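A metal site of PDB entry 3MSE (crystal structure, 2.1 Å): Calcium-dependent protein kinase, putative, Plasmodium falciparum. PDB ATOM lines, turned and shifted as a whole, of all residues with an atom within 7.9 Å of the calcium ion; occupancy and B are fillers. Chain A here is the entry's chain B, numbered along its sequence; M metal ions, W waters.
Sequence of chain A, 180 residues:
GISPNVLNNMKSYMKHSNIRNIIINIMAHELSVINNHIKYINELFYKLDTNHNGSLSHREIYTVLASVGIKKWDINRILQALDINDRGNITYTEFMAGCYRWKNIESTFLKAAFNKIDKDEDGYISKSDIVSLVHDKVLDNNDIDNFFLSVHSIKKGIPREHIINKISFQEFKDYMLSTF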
ATOM      1  N   PHE A 114       0.941  17.961  -3.519  1.00  0.00           N
ATOM      2  CA  PHE A 114       0.950  17.194  -4.751  1.00  0.00           C
ATOM      3  C   PHE A 114       2.113  17.602  -5.661  1.00  0.00           C
ATOM      4  O   PHE A 114       2.812  16.749  -6.182  1.00  0.00           O
ATOM      5  CB  PHE A 114      -0.380  17.376  -5.489  1.00  0.00           C
ATOM      6  CG  PHE A 114      -0.487  16.607  -6.767  1.00  0.00           C
ATOM      7  CD1 PHE A 114      -1.037  15.332  -6.774  1.00  0.00           C
ATOM      8  CD2 PHE A 114      -0.026  17.145  -7.968  1.00  0.00           C
ATOM      9  CE1 PHE A 114      -1.132  14.599  -7.948  1.00  0.00           C
ATOM     10  CE2 PHE A 114      -0.120  16.424  -9.168  1.00  0.00           C
ATOM     11  CZ  PHE A 114      -0.666  15.149  -9.151  1.00  0.00           C
ATOM     12  N   ASN A 115       2.317  18.912  -5.829  1.00  0.00           N
ATOM     13  CA  ASN A 115       3.381  19.426  -6.687  1.00  0.00           C
ATOM     14  C   ASN A 115       4.759  19.039  -6.191  1.00  0.00           C
ATOM     15  O   ASN A 115       5.622  18.703  -6.991  1.00  0.00           O
ATOM     16  CB  ASN A 115       3.278  20.936  -6.871  1.00  0.00           C
ATOM     17  CG  ASN A 115       2.196  21.340  -7.859  1.00  0.00           C
ATOM     18  OD1 ASN A 115       1.800  20.545  -8.719  1.00  0.00           O
ATOM     19  ND2 ASN A 115       1.698  22.558  -7.733  1.00  0.00           N
ATOM     20  N   ILE A 117       5.422  16.334  -4.552  1.00  0.00           N
ATOM     21  CA  ILE A 117       5.556  14.896  -4.755  1.00  0.00           C
ATOM     22  C   ILE A 117       5.811  14.517  -6.228  1.00  0.00           C
ATOM     23  O   ILE A 117       6.573  13.612  -6.520  1.00  0.00           O
ATOM     24  CB  ILE A 117       4.347  14.112  -4.173  1.00  0.00           C
ATOM     25  CG1 ILE A 117       4.263  14.311  -2.643  1.00  0.00           C
ATOM     26  CG2 ILE A 117       4.459  12.632  -4.499  1.00  0.00           C
ATOM     27  CD1 ILE A 117       2.902  13.927  -2.038  1.00  0.00           C
ATOM     28  N   ASP A 118       5.137  15.231  -7.133  1.00  0.00           N
ATOM     29  CA  ASP A 118       5.312  15.049  -8.565  1.00  0.00           C
ATOM     30  C   ASP A 118       6.646  15.678  -8.977  1.00  0.00           C
ATOM     31  O   ASP A 118       6.691  16.826  -9.442  1.00  0.00           O
ATOM     32  CB  ASP A 118       4.130  15.724  -9.265  1.00  0.00           C
ATOM     33  CG  ASP A 118       4.230  15.702 -10.774  1.00  0.00           C
ATOM     34  OD1 ASP A 118       3.583  16.578 -11.390  1.00  0.00           O
ATOM     35  OD2 ASP A 118       4.920  14.819 -11.334  1.00  0.00           O
ATOM     36  N   LYS A 119       7.742  14.948  -8.761  1.00  0.00           N
ATOM     37  CA  LYS A 119       9.092  15.497  -8.936  1.00  0.00           C
ATOM     38  C   LYS A 119       9.288  16.107 -10.321  1.00  0.00           C
ATOM     39  O   LYS A 119       9.850  17.200 -10.454  1.00  0.00           O
ATOM     40  CB  LYS A 119      10.181  14.426  -8.702  1.00  0.00           C
ATOM     41  CG  LYS A 119      10.421  14.017  -7.253  1.00  0.00           C
ATOM     42  CD  LYS A 119      11.278  12.725  -7.182  1.00  0.00           C
ATOM     43  CE  LYS A 119      12.801  12.973  -7.060  1.00  0.00           C
ATOM     44  NZ  LYS A 119      13.676  11.723  -6.796  1.00  0.00           N
ATOM     45  N   ASP A 120       8.788  15.400 -11.340  1.00  0.00           N
ATOM     46  CA  ASP A 120       9.010  15.775 -12.741  1.00  0.00           C
ATOM     47  C   ASP A 120       7.911  16.640 -13.355  1.00  0.00           C
ATOM     48  O   ASP A 120       7.881  16.856 -14.570  1.00  0.00           O
ATOM     49  CB  ASP A 120       9.258  14.513 -13.582  1.00  0.00           C
ATOM     50  CG  ASP A 120      10.515  13.777 -13.172  1.00  0.00           C
ATOM     51  OD1 ASP A 120      11.572  14.420 -13.022  1.00  0.00           O
ATOM     52  OD2 ASP A 120      10.448  12.534 -12.988  1.00  0.00           O
ATOM     53  N   GLU A 121       7.008  17.144 -12.501  1.00  0.00           N
ATOM     54  CA  GLU A 121       5.991  18.131 -12.880  1.00  0.00           C
ATOM     55  C   GLU A 121       5.176  17.730 -14.102  1.00  0.00           C
ATOM     56  O   GLU A 121       4.794  18.579 -14.912  1.00  0.00           O
ATOM     57  CB  GLU A 121       6.626  19.508 -13.088  1.00  0.00           C
ATOM     58  CG  GLU A 121       7.445  19.986 -11.908  1.00  0.00           C
ATOM     59  CD  GLU A 121       8.194  21.271 -12.191  1.00  0.00           C
ATOM     60  OE1 GLU A 121       7.915  21.896 -13.242  1.00  0.00           O
ATOM     61  OE2 GLU A 121       9.055  21.655 -11.375  1.00  0.00           O
ATOM     62  N   ASP A 122       4.914  16.435 -14.227  1.00  0.00           N
ATOM     63  CA  ASP A 122       4.126  15.900 -15.338  1.00  0.00           C
ATOM     64  C   ASP A 122       2.617  15.838 -15.035  1.00  0.00           C
ATOM     65  O   ASP A 122       1.831  15.433 -15.881  1.00  0.00           O
ATOM     66  CB  ASP A 122       4.645  14.514 -15.730  1.00  0.00           C
ATOM     67  CG  ASP A 122       4.899  13.627 -14.522  1.00  0.00           C
ATOM     68  OD1 ASP A 122       6.089  13.443 -14.144  1.00  0.00           O
ATOM     69  OD2 ASP A 122       3.914  13.143 -13.928  1.00  0.00           O
ATOM     70  N   GLY A 123       2.226  16.224 -13.817  1.00  0.00           N
ATOM     71  CA  GLY A 123       0.819  16.200 -13.381  1.00  0.00           C
ATOM     72  C   GLY A 123       0.275  14.876 -12.854  1.00  0.00           C
ATOM     73  O   GLY A 123      -0.922  14.749 -12.580  1.00  0.00           O
ATOM     74  N   TYR A 124       1.147  13.879 -12.698  1.00  0.00           N
ATOM     75  CA  TYR A 124       0.746  12.590 -12.155  1.00  0.00           C
ATOM     76  C   TYR A 124       1.704  12.118 -11.072  1.00  0.00           C
ATOM     77  O   TYR A 124       2.923  12.250 -11.217  1.00  0.00           O
ATOM     78  CB  TYR A 124       0.652  11.547 -13.272  1.00  0.00           C
ATOM     79  CG  TYR A 124      -0.572  11.730 -14.169  1.00  0.00           C
ATOM     80  CD1 TYR A 124      -1.761  11.052 -13.905  1.00  0.00           C
ATOM     81  CD2 TYR A 124      -0.519  12.581 -15.275  1.00  0.00           C
ATOM     82  CE1 TYR A 124      -2.887  11.225 -14.715  1.00  0.00           C
ATOM     83  CE2 TYR A 124      -1.637  12.764 -16.103  1.00  0.00           C
ATOM     84  CZ  TYR A 124      -2.822  12.088 -15.815  1.00  0.00           C
ATOM     85  OH  TYR A 124      -3.926  12.253 -16.620  1.00  0.00           O
ATOM     86  N   ILE A 125       1.151  11.549  -9.986  1.00  0.00           N
ATOM     87  CA  ILE A 125       1.984  10.903  -8.977  1.00  0.00           C
ATOM     88  C   ILE A 125       2.187   9.426  -9.327  1.00  0.00           C
ATOM     89  O   ILE A 125       1.253   8.631  -9.214  1.00  0.00           O
ATOM     90  CB  ILE A 125       1.440  11.079  -7.522  1.00  0.00           C
ATOM     91  CG1 ILE A 125       1.651  12.516  -7.042  1.00  0.00           C
ATOM     92  CG2 ILE A 125       2.122  10.090  -6.558  1.00  0.00           C
ATOM     93  CD1 ILE A 125       1.033  12.822  -5.670  1.00  0.00           C
ATOM     94  N   SER A 126       3.400   9.090  -9.749  1.00  0.00           N
ATOM     95  CA  SER A 126       3.742   7.715 -10.106  1.00  0.00           C
ATOM     96  C   SER A 126       4.223   6.931  -8.900  1.00  0.00           C
ATOM     97  O   SER A 126       4.430   7.489  -7.818  1.00  0.00           O
ATOM     98  CB  SER A 126       4.827   7.682 -11.198  1.00  0.00           C
ATOM     99  OG  SER A 126       6.007   8.382 -10.794  1.00  0.00           O
ATOM    100  N   LYS A 127       4.390   5.639  -9.102  1.00  0.00           N
ATOM    101  CA  LYS A 127       4.975   4.768  -8.112  1.00  0.00           C
ATOM    102  C   LYS A 127       6.375   5.272  -7.710  1.00  0.00           C
ATOM    103  O   LYS A 127       6.715   5.316  -6.512  1.00  0.00           O
ATOM    104  CB  LYS A 127       5.045   3.347  -8.670  1.00  0.00           C
ATOM    105  CG  LYS A 127       5.040   2.255  -7.628  1.00  0.00           C
ATOM    106  CD  LYS A 127       6.450   1.781  -7.297  1.00  0.00           C
ATOM    107  CE  LYS A 127       6.458   0.687  -6.240  1.00  0.00           C
ATOM    108  NZ  LYS A 127       5.828  -0.577  -6.724  1.00  0.00           N
ATOM    109  N   SER A 128       7.164   5.695  -8.696  1.00  0.00           N
ATOM    110  CA  SER A 128       8.517   6.180  -8.432  1.00  0.00           C
ATOM    111  C   SER A 128       8.527   7.513  -7.652  1.00  0.00           C
ATOM    112  O   SER A 128       9.451   7.794  -6.897  1.00  0.00           O
ATOM    113  CB  SER A 128       9.357   6.265  -9.716  1.00  0.00           C
ATOM    114  OG  SER A 128       9.151   7.485 -10.404  1.00  0.00           O
ATOM    115  N   ASP A 129       7.488   8.324  -7.835  1.00  0.00           N
ATOM    116  CA  ASP A 129       7.365   9.553  -7.041  1.00  0.00           C
ATOM    117  C   ASP A 129       7.169   9.254  -5.541  1.00  0.00           C
ATOM    118  O   ASP A 129       7.669  10.013  -4.684  1.00  0.00           O
ATOM    119  CB  ASP A 129       6.209  10.402  -7.556  1.00  0.00           C
ATOM    120  CG  ASP A 129       6.537  11.071  -8.883  1.00  0.00           C
ATOM    121  OD1 ASP A 129       7.713  11.426  -9.120  1.00  0.00           O
ATOM    122  OD2 ASP A 129       5.601  11.270  -9.678  1.00  0.00           O
ATOM    123  N   LYS A 166      -1.098   5.408 -11.463  1.00  0.00           N
ATOM    124  CA  LYS A 166      -0.704   6.791 -11.367  1.00  0.00           C
ATOM    125  C   LYS A 166      -1.830   7.529 -10.672  1.00  0.00           C
ATOM    126  O   LYS A 166      -2.955   7.021 -10.590  1.00  0.00           O
ATOM    127  CB  LYS A 166      -0.495   7.388 -12.764  1.00  0.00           C
ATOM    128  CG  LYS A 166       0.355   6.519 -13.700  1.00  0.00           C
ATOM    129  CD  LYS A 166       0.614   7.209 -15.043  1.00  0.00           C
ATOM    130  CE  LYS A 166       1.776   8.186 -14.957  1.00  0.00           C
ATOM    131  NZ  LYS A 166       3.063   7.502 -14.669  1.00  0.00           N
ATOM    132  N   ILE A 167      -1.554   8.727 -10.176  1.00  0.00           N
ATOM    133  CA  ILE A 167      -2.542   9.491  -9.423  1.00  0.00           C
ATOM    134  C   ILE A 167      -2.604  10.936  -9.910  1.00  0.00           C
ATOM    135  O   ILE A 167      -1.605  11.657  -9.867  1.00  0.00           O
ATOM    136  CB  ILE A 167      -2.228   9.441  -7.887  1.00  0.00           C
ATOM    137  CG1 ILE A 167      -2.254   7.999  -7.364  1.00  0.00           C
ATOM    138  CG2 ILE A 167      -3.195  10.321  -7.101  1.00  0.00           C
ATOM    139  CD1 ILE A 167      -1.638   7.817  -5.967  1.00  0.00           C
HETATM  140 CA    CA M   1       5.224  12.563 -11.781  1.00  0.00          CA
HETATM  141  O   HOH W   1       5.575  10.720 -12.453  1.00  0.00           O
HETATM  142  O   HOH W   2       7.469  13.038 -11.488  1.00  0.00           O
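The backbone NH of Gly 123 is in hydrogen-bond range of the side-chain carboxylate of Asp 118 (2.8 Å). N of Asp 129 is in hydrogen-bond range of OG of Ser 126, 3.3 Å away. OD2 of Asp 118 sits close to N of Glu 121 (3.3 Å).
Of the 17 residues printed, 4 come within 4 Å of the calcium ion.
The calcium ion is bound by water W1 (2.0 Å). The calcium ion is bound by water W2 (2.3 Å). OD2 of Asp 118 binds the calcium ion (2.3 Å). O of Tyr 124 is bound to the calcium ion (2.4 Å). The calcium ion is bound by OD2 of Asp 129 (2.5 Å). OD2 of Asp 122 binds the calcium ion, 2.6 Å away. The calcium ion is bound by OD1 of Asp 122. The calcium ion has seven donor atoms within binding distance.
Water W2 lies within hydrogen-bond range of the backbone NH of Asp 120 (2.7 Å), the side-chain carboxylate of Asp 129 (2.9 Å) and the backbone NH of Lys 119 (3.3 Å).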
